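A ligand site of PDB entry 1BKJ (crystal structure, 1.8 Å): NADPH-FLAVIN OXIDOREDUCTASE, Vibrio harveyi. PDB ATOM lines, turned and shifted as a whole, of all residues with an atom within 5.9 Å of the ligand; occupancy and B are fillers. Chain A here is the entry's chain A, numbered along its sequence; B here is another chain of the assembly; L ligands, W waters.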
ATOM      1  N   HIS A  11      -5.274  16.724   3.987  1.00  0.00           N
ATOM      2  CA  HIS A  11      -4.241  16.394   4.974  1.00  0.00           C
ATOM      3  C   HIS A  11      -3.781  17.542   5.870  1.00  0.00           C
ATOM      4  O   HIS A  11      -3.563  18.648   5.408  1.00  0.00           O
ATOM      5  CB  HIS A  11      -2.991  15.776   4.302  1.00  0.00           C
ATOM      6  CG  HIS A  11      -1.776  15.683   5.191  1.00  0.00           C
ATOM      7  ND1 HIS A  11      -1.661  14.745   6.194  1.00  0.00           N
ATOM      8  CD2 HIS A  11      -0.690  16.490   5.309  1.00  0.00           C
ATOM      9  CE1 HIS A  11      -0.558  14.968   6.886  1.00  0.00           C
ATOM     10  NE2 HIS A  11       0.045  16.026   6.377  1.00  0.00           N
ATOM     11  N   ARG A  12      -3.586  17.189   7.130  1.00  0.00           N
ATOM     12  CA  ARG A  12      -2.954  18.031   8.147  1.00  0.00           C
ATOM     13  C   ARG A  12      -2.415  17.047   9.181  1.00  0.00           C
ATOM     14  O   ARG A  12      -3.012  15.975   9.391  1.00  0.00           O
ATOM     15  CB  ARG A  12      -3.831  19.179   8.738  1.00  0.00           C
ATOM     16  CG  ARG A  12      -5.068  18.800   9.394  1.00  0.00           C
ATOM     17  CD  ARG A  12      -6.262  19.019   8.473  1.00  0.00           C
ATOM     18  NE  ARG A  12      -7.141  17.872   8.563  1.00  0.00           N
ATOM     19  CZ  ARG A  12      -7.878  17.570   9.633  1.00  0.00           C
ATOM     20  NH1 ARG A  12      -7.861  18.352  10.716  1.00  0.00           N
ATOM     21  NH2 ARG A  12      -8.563  16.446   9.688  1.00  0.00           N
ATOM     22  N   SER A  13      -1.238  17.346   9.719  1.00  0.00           N
ATOM     23  CA  SER A  13      -0.619  16.500  10.730  1.00  0.00           C
ATOM     24  C   SER A  13      -1.391  16.632  12.033  1.00  0.00           C
ATOM     25  O   SER A  13      -1.805  17.731  12.402  1.00  0.00           O
ATOM     26  CB  SER A  13       0.833  16.867  10.955  1.00  0.00           C
ATOM     27  OG  SER A  13       1.601  16.556   9.799  1.00  0.00           O
ATOM     28  N   ARG A  15      -1.478  15.788  16.043  1.00  0.00           N
ATOM     29  CA  ARG A  15      -0.588  15.606  17.167  1.00  0.00           C
ATOM     30  C   ARG A  15      -1.290  15.425  18.522  1.00  0.00           C
ATOM     31  O   ARG A  15      -0.665  15.588  19.567  1.00  0.00           O
ATOM     32  CB  ARG A  15       0.410  16.772  17.202  1.00  0.00           C
ATOM     33  CG  ARG A  15       1.378  16.810  16.021  1.00  0.00           C
ATOM     34  CD  ARG A  15       2.252  18.047  16.043  1.00  0.00           C
ATOM     35  NE  ARG A  15       3.097  18.165  14.851  1.00  0.00           N
ATOM     36  CZ  ARG A  15       2.784  18.858  13.758  1.00  0.00           C
ATOM     37  NH1 ARG A  15       1.636  19.510  13.688  1.00  0.00           N
ATOM     38  NH2 ARG A  15       3.626  18.914  12.748  1.00  0.00           N
ATOM     39  N   ALA A  64      12.551  10.886  20.572  1.00  0.00           N
ATOM     40  CA  ALA A  64      12.013  11.704  19.494  1.00  0.00           C
ATOM     41  C   ALA A  64      12.064  13.191  19.856  1.00  0.00           C
ATOM     42  O   ALA A  64      11.723  14.047  19.037  1.00  0.00           O
ATOM     43  CB  ALA A  64      10.576  11.291  19.182  1.00  0.00           C
ATOM     44  N   GLN A  67       8.273  14.136  22.356  1.00  0.00           N
ATOM     45  CA  GLN A  67       7.060  14.351  21.576  1.00  0.00           C
ATOM     46  C   GLN A  67       6.044  13.361  22.142  1.00  0.00           C
ATOM     47  O   GLN A  67       6.099  12.165  21.829  1.00  0.00           O
ATOM     48  CB  GLN A  67       7.332  14.140  20.076  1.00  0.00           C
ATOM     49  CG  GLN A  67       8.384  15.124  19.513  1.00  0.00           C
ATOM     50  CD  GLN A  67       8.454  15.112  17.998  1.00  0.00           C
ATOM     51  OE1 GLN A  67       7.464  15.350  17.325  1.00  0.00           O
ATOM     52  NE2 GLN A  67       9.641  14.853  17.446  1.00  0.00           N
ATOM     53  N   TYR A  69       2.879  12.644  21.755  1.00  0.00           N
ATOM     54  CA  TYR A  69       1.996  11.898  20.877  1.00  0.00           C
ATOM     55  C   TYR A  69       2.566  10.573  20.343  1.00  0.00           C
ATOM     56  O   TYR A  69       1.858   9.777  19.735  1.00  0.00           O
ATOM     57  CB  TYR A  69       1.480  12.787  19.743  1.00  0.00           C
ATOM     58  CG  TYR A  69       2.442  13.830  19.252  1.00  0.00           C
ATOM     59  CD1 TYR A  69       2.535  15.076  19.928  1.00  0.00           C
ATOM     60  CD2 TYR A  69       3.269  13.596  18.132  1.00  0.00           C
ATOM     61  CE1 TYR A  69       3.445  16.077  19.484  1.00  0.00           C
ATOM     62  CE2 TYR A  69       4.187  14.589  17.681  1.00  0.00           C
ATOM     63  CZ  TYR A  69       4.266  15.820  18.370  1.00  0.00           C
ATOM     64  OH  TYR A  69       5.134  16.796  17.951  1.00  0.00           O
ATOM     65  N   VAL A 127       1.010  11.606  11.911  1.00  0.00           N
ATOM     66  CA  VAL A 127       2.130  12.521  11.801  1.00  0.00           C
ATOM     67  C   VAL A 127       3.414  11.712  11.697  1.00  0.00           C
ATOM     68  O   VAL A 127       3.580  10.725  12.400  1.00  0.00           O
ATOM     69  CB  VAL A 127       2.185  13.542  13.010  1.00  0.00           C
ATOM     70  CG1 VAL A 127       2.421  12.847  14.349  1.00  0.00           C
ATOM     71  CG2 VAL A 127       3.250  14.635  12.773  1.00  0.00           C
ATOM     72  N   TYR A 128       4.301  12.138  10.802  1.00  0.00           N
ATOM     73  CA  TYR A 128       5.593  11.484  10.648  1.00  0.00           C
ATOM     74  C   TYR A 128       6.473  11.966  11.795  1.00  0.00           C
ATOM     75  O   TYR A 128       6.254  13.070  12.303  1.00  0.00           O
ATOM     76  CB  TYR A 128       6.277  11.911   9.356  1.00  0.00           C
ATOM     77  CG  TYR A 128       5.760  11.340   8.073  1.00  0.00           C
ATOM     78  CD1 TYR A 128       4.673  11.916   7.409  1.00  0.00           C
ATOM     79  CD2 TYR A 128       6.384  10.216   7.496  1.00  0.00           C
ATOM     80  CE1 TYR A 128       4.210  11.408   6.172  1.00  0.00           C
ATOM     81  CE2 TYR A 128       5.933   9.696   6.259  1.00  0.00           C
ATOM     82  CZ  TYR A 128       4.845  10.295   5.617  1.00  0.00           C
ATOM     83  OH  TYR A 128       4.374   9.823   4.435  1.00  0.00           O
ATOM     84  N   ILE A 129       7.415  11.138  12.253  1.00  0.00           N
ATOM     85  CA  ILE A 129       8.317  11.484  13.357  1.00  0.00           C
ATOM     86  C   ILE A 129       9.783  11.282  12.919  1.00  0.00           C
ATOM     87  O   ILE A 129      10.337  10.189  13.068  1.00  0.00           O
ATOM     88  CB  ILE A 129       8.000  10.665  14.678  1.00  0.00           C
ATOM     89  CG1 ILE A 129       6.525  10.816  15.112  1.00  0.00           C
ATOM     90  CG2 ILE A 129       8.947  11.083  15.835  1.00  0.00           C
ATOM     91  CD1 ILE A 129       6.082  12.207  15.507  1.00  0.00           C
ATOM     92  N   GLY A 130      10.386  12.347  12.390  1.00  0.00           N
ATOM     93  CA  GLY A 130      11.769  12.300  11.963  1.00  0.00           C
ATOM     94  C   GLY A 130      12.726  12.605  13.105  1.00  0.00           C
ATOM     95  O   GLY A 130      13.935  12.418  12.981  1.00  0.00           O
ATOM     96  N   GLY A 131      12.154  13.056  14.225  1.00  0.00           N
ATOM     97  CA  GLY A 131      12.895  13.383  15.432  1.00  0.00           C
ATOM     98  C   GLY A 131      13.722  12.246  16.019  1.00  0.00           C
ATOM     99  O   GLY A 131      14.685  12.500  16.726  1.00  0.00           O
ATOM    100  N   LEU A 132      13.341  11.003  15.705  1.00  0.00           N
ATOM    101  CA  LEU A 132      14.053   9.811  16.150  1.00  0.00           C
ATOM    102  C   LEU A 132      15.508   9.770  15.712  1.00  0.00           C
ATOM    103  O   LEU A 132      16.356   9.183  16.391  1.00  0.00           O
ATOM    104  CB  LEU A 132      13.356   8.543  15.610  1.00  0.00           C
ATOM    105  CG  LEU A 132      12.002   8.141  16.187  1.00  0.00           C
ATOM    106  CD1 LEU A 132      11.509   6.860  15.496  1.00  0.00           C
ATOM    107  CD2 LEU A 132      12.121   7.933  17.692  1.00  0.00           C
ATOM    108  N   ARG A 133      15.799  10.439  14.585  1.00  0.00           N
ATOM    109  CA  ARG A 133      17.169  10.496  14.015  1.00  0.00           C
ATOM    110  C   ARG A 133      18.188  11.271  14.857  1.00  0.00           C
ATOM    111  O   ARG A 133      19.392  11.006  14.777  1.00  0.00           O
ATOM    112  CB  ARG A 133      17.160  11.022  12.569  1.00  0.00           C
ATOM    113  CG  ARG A 133      16.555  10.043  11.567  1.00  0.00           C
ATOM    114  CD  ARG A 133      16.973  10.344  10.112  1.00  0.00           C
ATOM    115  NE  ARG A 133      16.685  11.720   9.707  1.00  0.00           N
ATOM    116  CZ  ARG A 133      15.509  12.175   9.295  1.00  0.00           C
ATOM    117  NH1 ARG A 133      14.439  11.386   9.211  1.00  0.00           N
ATOM    118  NH2 ARG A 133      15.382  13.455   8.992  1.00  0.00           N
ATOM    119  N   PHE A 153      12.495   7.043  10.163  1.00  0.00           N
ATOM    120  CA  PHE A 153      11.470   7.855  10.818  1.00  0.00           C
ATOM    121  C   PHE A 153      10.388   6.973  11.402  1.00  0.00           C
ATOM    122  O   PHE A 153      10.286   5.790  11.071  1.00  0.00           O
ATOM    123  CB  PHE A 153      10.844   8.893   9.840  1.00  0.00           C
ATOM    124  CG  PHE A 153      10.290   8.301   8.569  1.00  0.00           C
ATOM    125  CD1 PHE A 153       8.980   7.795   8.513  1.00  0.00           C
ATOM    126  CD2 PHE A 153      11.090   8.210   7.414  1.00  0.00           C
ATOM    127  CE1 PHE A 153       8.469   7.193   7.348  1.00  0.00           C
ATOM    128  CE2 PHE A 153      10.600   7.604   6.223  1.00  0.00           C
ATOM    129  CZ  PHE A 153       9.282   7.099   6.196  1.00  0.00           C
ATOM    130  N   GLU A 165      -5.954  23.644  10.871  1.00  0.00           N
ATOM    131  CA  GLU A 165      -6.272  24.142   9.543  1.00  0.00           C
ATOM    132  C   GLU A 165      -5.170  23.676   8.603  1.00  0.00           C
ATOM    133  O   GLU A 165      -4.051  23.411   9.039  1.00  0.00           O
ATOM    134  CB  GLU A 165      -6.404  25.669   9.574  1.00  0.00           C
ATOM    135  N   LYS A 167      -2.238  23.703   6.154  1.00  0.00           N
ATOM    136  CA  LYS A 167      -1.077  24.583   6.008  1.00  0.00           C
ATOM    137  C   LYS A 167      -0.743  24.865   4.543  1.00  0.00           C
ATOM    138  O   LYS A 167      -0.629  23.939   3.742  1.00  0.00           O
ATOM    139  CB  LYS A 167       0.137  23.931   6.669  1.00  0.00           C
ATOM    140  CG  LYS A 167       0.740  24.724   7.778  1.00  0.00           C
ATOM    141  CD  LYS A 167       2.167  24.297   8.091  1.00  0.00           C
ATOM    142  CE  LYS A 167       2.330  23.828   9.537  1.00  0.00           C
ATOM    143  NZ  LYS A 167       3.781  23.723   9.896  1.00  0.00           N
ATOM    144  N   ARG A 169       1.361  25.743   1.137  1.00  0.00           N
ATOM    145  CA  ARG A 169       2.701  25.411   0.655  1.00  0.00           C
ATOM    146  C   ARG A 169       3.131  26.448  -0.349  1.00  0.00           C
ATOM    147  O   ARG A 169       2.326  27.286  -0.756  1.00  0.00           O
ATOM    148  CB  ARG A 169       2.717  24.053  -0.065  1.00  0.00           C
ATOM    149  CG  ARG A 169       3.098  22.861   0.788  1.00  0.00           C
ATOM    150  CD  ARG A 169       2.001  22.471   1.739  1.00  0.00           C
ATOM    151  NE  ARG A 169       2.219  21.144   2.299  1.00  0.00           N
ATOM    152  CZ  ARG A 169       1.810  20.762   3.497  1.00  0.00           C
ATOM    153  NH1 ARG A 169       1.157  21.602   4.288  1.00  0.00           N
ATOM    154  NH2 ARG A 169       2.042  19.534   3.921  1.00  0.00           N
ATOM    155  N   ALA B  36       0.511  18.875  -1.340  1.00  0.00           N
ATOM    156  CA  ALA B  36      -0.236  18.603  -0.107  1.00  0.00           C
ATOM    157  C   ALA B  36       0.438  17.579   0.813  1.00  0.00           C
ATOM    158  O   ALA B  36      -0.011  17.350   1.951  1.00  0.00           O
ATOM    159  CB  ALA B  36      -1.644  18.169  -0.431  1.00  0.00           C
ATOM    160  N   ALA B  37       1.537  16.996   0.334  1.00  0.00           N
ATOM    161  CA  ALA B  37       2.308  16.006   1.095  1.00  0.00           C
ATOM    162  C   ALA B  37       3.047  16.643   2.273  1.00  0.00           C
ATOM    163  O   ALA B  37       3.421  17.815   2.212  1.00  0.00           O
ATOM    164  CB  ALA B  37       3.309  15.324   0.169  1.00  0.00           C
ATOM    165  N   SER B  38       3.261  15.865   3.337  1.00  0.00           N
ATOM    166  CA  SER B  38       3.987  16.317   4.530  1.00  0.00           C
ATOM    167  C   SER B  38       5.410  16.706   4.152  1.00  0.00           C
ATOM    168  O   SER B  38       5.948  16.177   3.176  1.00  0.00           O
ATOM    169  CB  SER B  38       4.049  15.197   5.584  1.00  0.00           C
ATOM    170  OG  SER B  38       2.773  14.837   6.077  1.00  0.00           O
ATOM    171  N   SER B  39       5.992  17.635   4.905  1.00  0.00           N
ATOM    172  CA  SER B  39       7.339  18.133   4.636  1.00  0.00           C
ATOM    173  C   SER B  39       8.127  18.207   5.944  1.00  0.00           C
ATOM    174  O   SER B  39       7.643  18.783   6.922  1.00  0.00           O
ATOM    175  CB  SER B  39       7.246  19.523   3.975  1.00  0.00           C
ATOM    176  OG  SER B  39       8.527  20.104   3.763  1.00  0.00           O
ATOM    177  N   SER B  40       9.322  17.601   5.958  1.00  0.00           N
ATOM    178  CA  SER B  40      10.223  17.596   7.125  1.00  0.00           C
ATOM    179  C   SER B  40      10.583  19.011   7.532  1.00  0.00           C
ATOM    180  O   SER B  40      11.162  19.746   6.736  1.00  0.00           O
ATOM    181  CB  SER B  40      11.514  16.844   6.822  1.00  0.00           C
ATOM    182  OG  SER B  40      11.278  15.521   6.386  1.00  0.00           O
ATOM    183  N   SER B  41      10.184  19.394   8.760  1.00  0.00           N
ATOM    184  CA  SER B  41      10.431  20.733   9.330  1.00  0.00           C
ATOM    185  C   SER B  41       9.920  21.891   8.461  1.00  0.00           C
ATOM    186  O   SER B  41      10.395  23.024   8.571  1.00  0.00           O
ATOM    187  CB  SER B  41      11.920  20.928   9.671  1.00  0.00           C
ATOM    188  OG  SER B  41      12.384  19.929  10.558  1.00  0.00           O
ATOM    189  N   MET B  42       8.958  21.566   7.592  1.00  0.00           N
ATOM    190  CA  MET B  42       8.349  22.499   6.634  1.00  0.00           C
ATOM    191  C   MET B  42       9.446  23.145   5.716  1.00  0.00           C
ATOM    192  O   MET B  42       9.254  24.235   5.154  1.00  0.00           O
ATOM    193  CB  MET B  42       7.458  23.541   7.383  1.00  0.00           C
ATOM    194  CG  MET B  42       6.397  24.259   6.545  1.00  0.00           C
ATOM    195  SD  MET B  42       5.428  23.120   5.601  1.00  0.00           S
ATOM    196  CE  MET B  42       4.196  24.190   4.939  1.00  0.00           C
ATOM    197  N   VAL B 106      13.616  11.167   1.298  1.00  0.00           N
ATOM    198  CA  VAL B 106      12.366  10.750   1.946  1.00  0.00           C
ATOM    199  C   VAL B 106      11.205  11.645   1.488  1.00  0.00           C
ATOM    200  O   VAL B 106      10.202  11.122   1.018  1.00  0.00           O
ATOM    201  CB  VAL B 106      12.460  10.767   3.519  1.00  0.00           C
ATOM    202  CG1 VAL B 106      11.083  10.607   4.171  1.00  0.00           C
ATOM    203  CG2 VAL B 106      13.370   9.644   4.007  1.00  0.00           C
ATOM    204  N   ASP B 107      11.388  12.967   1.579  1.00  0.00           N
ATOM    205  CA  ASP B 107      10.350  13.947   1.174  1.00  0.00           C
ATOM    206  C   ASP B 107       9.951  13.856  -0.302  1.00  0.00           C
ATOM    207  O   ASP B 107       8.783  14.075  -0.621  1.00  0.00           O
ATOM    208  CB  ASP B 107      10.765  15.366   1.554  1.00  0.00           C
ATOM    209  CG  ASP B 107      10.706  15.636   3.059  1.00  0.00           C
ATOM    210  OD1 ASP B 107      10.653  14.703   3.890  1.00  0.00           O
ATOM    211  OD2 ASP B 107      10.711  16.822   3.444  1.00  0.00           O
ATOM    212  N   ILE B 110       7.639  10.748  -0.699  1.00  0.00           N
ATOM    213  CA  ILE B 110       6.316  11.091  -0.160  1.00  0.00           C
ATOM    214  C   ILE B 110       5.535  11.937  -1.181  1.00  0.00           C
ATOM    215  O   ILE B 110       4.379  11.627  -1.481  1.00  0.00           O
ATOM    216  CB  ILE B 110       6.427  11.870   1.172  1.00  0.00           C
ATOM    217  CG1 ILE B 110       7.099  10.998   2.240  1.00  0.00           C
ATOM    218  CG2 ILE B 110       5.043  12.281   1.687  1.00  0.00           C
ATOM    219  CD1 ILE B 110       7.503  11.718   3.499  1.00  0.00           C
HETATM  220  N1  LIG L   1       6.090  16.629  12.866  1.00  0.00           N
HETATM  221  C1  LIG L   1       6.271  16.562  14.225  1.00  0.00           C
HETATM  222  O1  LIG L   1       5.613  17.160  15.041  1.00  0.00           O
HETATM  223  N2  LIG L   1       7.363  15.782  14.587  1.00  0.00           N
HETATM  224  C2  LIG L   1       8.375  15.277  13.727  1.00  0.00           C
HETATM  225  O2  LIG L   1       9.329  14.726  14.243  1.00  0.00           O
HETATM  226  C3  LIG L   1       8.144  15.490  12.333  1.00  0.00           C
HETATM  227  N3  LIG L   1       8.959  14.778  11.459  1.00  0.00           N
HETATM  228  C4  LIG L   1       8.642  14.701  10.101  1.00  0.00           C
HETATM  229  C5  LIG L   1       9.407  13.859   9.309  1.00  0.00           C
HETATM  230  C6  LIG L   1       9.104  13.689   7.967  1.00  0.00           C
HETATM  231  C7  LIG L   1       9.879  12.571   7.202  1.00  0.00           C
HETATM  232  C8  LIG L   1       8.026  14.416   7.384  1.00  0.00           C
HETATM  233  C9  LIG L   1       7.702  14.394   5.933  1.00  0.00           C
HETATM  234  C10 LIG L   1       7.254  15.243   8.161  1.00  0.00           C
HETATM  235  C11 LIG L   1       7.536  15.409   9.550  1.00  0.00           C
HETATM  236  N4  LIG L   1       6.728  16.187  10.447  1.00  0.00           N
HETATM  237  C12 LIG L   1       6.960  16.164  11.846  1.00  0.00           C
HETATM  238  C13 LIG L   1       5.540  16.736  10.044  1.00  0.00           C
HETATM  239  C14 LIG L   1       5.525  18.212   9.725  1.00  0.00           C
HETATM  240  O3  LIG L   1       6.234  19.120  10.438  1.00  0.00           O
HETATM  241  C15 LIG L   1       4.635  18.658   8.636  1.00  0.00           C
HETATM  242  O4  LIG L   1       4.409  17.749   7.590  1.00  0.00           O
HETATM  243  C16 LIG L   1       4.493  20.100   8.239  1.00  0.00           C
HETATM  244  O5  LIG L   1       4.965  21.112   9.098  1.00  0.00           O
HETATM  245  C17 LIG L   1       3.546  20.500   7.211  1.00  0.00           C
HETATM  246  O6  LIG L   1       2.285  20.444   7.927  1.00  0.00           O
HETATM  247  P1  LIG L   1       1.077  19.384   7.626  1.00  0.00           P
HETATM  248  O7  LIG L   1       0.598  19.785   6.322  1.00  0.00           O
HETATM  249  O8  LIG L   1       0.172  19.581   8.786  1.00  0.00           O
HETATM  250  O9  LIG L   1       1.649  18.027   7.488  1.00  0.00           O
HETATM  251  O   HOH W   1      -1.587  21.649   9.491  1.00  0.00           O
HETATM  252  O   HOH W   2      -1.885  20.788   6.065  1.00  0.00           O
HETATM  253  O   HOH W   3       1.861  20.739  10.943  1.00  0.00           O
HETATM  254  O   HOH W   4      12.617  14.186   8.632  1.00  0.00           O
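The side-chain amide oxygen (OE1) of Gln 67 is in hydrogen-bond range of the side-chain hydroxyl (OH) of Tyr 69 (2.8 Å).
The side-chain amide nitrogen (NE2) of Gln 67 sits at hydrogen-bond distance from the backbone carbonyl oxygen (O) of Ala 64 (2.7 Å).
The guanidinium group (NH1) of Arg 169 is in hydrogen-bond range of the backbone carbonyl oxygen (O) of Lys 167 (3.0 Å).
NH2 of Arg 169 sits at hydrogen-bond distance from O of Ala 37 of chain B, 2.8 Å away.
A ring nitrogen (NE2) of His 11 sits at hydrogen-bond distance from the side-chain hydroxyl (OG) of Ser 38 of chain B, 3.0 Å away.
OG of Ser 40 of chain B lies within hydrogen-bond range of OD1 of Asp 107 of chain B (2.7 Å).
Water W2 lies within hydrogen-bond range of an oxygen (O7) of the ligand, the backbone carbonyl oxygen of His 11 and the backbone NH of Lys 167.
Water W1 bridges O8 of the ligand and O of Glu 165.
Water W3 lies within hydrogen-bond range of an oxygen (O8) of the ligand (3.0 Å) and the guanidinium group (NH1) of Arg 15 (3.0 Å).
Water W4 lies within hydrogen-bond range of NH2 of Arg 133 (2.9 Å) and OG of Ser 40 of chain B (2.9 Å).
The backbone carbonyl oxygen of Tyr 128 lies close to a nitrogen (N3) of the ligand.
Residues that only touch the ligand: Ser 40 of chain B, Ser 38 of chain B, Val 127, Ile 129, Arg 12, Asp 107 of chain B, Met 42 of chain B, Ile 110 of chain B and Val 106 of chain B.
Hydrophobic or aromatic side chains that line the ligand: His 11, Tyr 69, Val 127, Tyr 128, Ile 129, Met 42 of chain B, Val 106 of chain B and Ile 110 of chain B.
20 residues have an atom within 4 Å of the ligand: His 11, Arg 12, Ser 13, Arg 15, Gln 67, Tyr 69, Val 127, Tyr 128, Ile 129, Gly 130, Gly 131, Lys 167, Arg 169, Ser 38 of chain B, Ser 39 of chain B, Ser 40 of chain B, Met 42 of chain B, Val 106 of chain B, Asp 107 of chain B and Ile 110 of chain B.
An oxygen (O1) of the ligand is in hydrogen-bond range of the guanidinium group (NE) of Arg 15, 2.7 Å away.
The backbone NH (N) of Ser 13 lies within hydrogen-bond range of an oxygen (O8) of the ligand.
O9 of the ligand sits at hydrogen-bond distance from OG of Ser 13 (2.7 Å).
OE1 of Gln 67 sits at hydrogen-bond distance from N2 of the ligand.
The guanidinium group of Arg 169 is in salt-bridge range of an oxygen (O7) of the ligand (2.8 Å).
NE2 of His 11 sits at hydrogen-bond distance from O9 of the ligand.
A nitrogen (N3) of the ligand lies within hydrogen-bond range of the backbone NH of Gly 130 (3.0 Å).
OH of Tyr 69 is in hydrogen-bond range of O1 of the ligand (3.0 Å).
An oxygen (O5) of the ligand lies within hydrogen-bond range of the side-chain amino group (NZ) of Lys 167, 3.0 Å away.
An oxygen (O4) of the ligand is in hydrogen-bond range of the backbone NH (N) of Ser 39 of chain B, 3.1 Å away.
O4 of the ligand is in hydrogen-bond range of O of Ser 39 of chain B (3.5 Å).
An oxygen (O2) of the ligand sits at hydrogen-bond distance from the backbone NH (N) of Gly 131 (3.3 Å).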
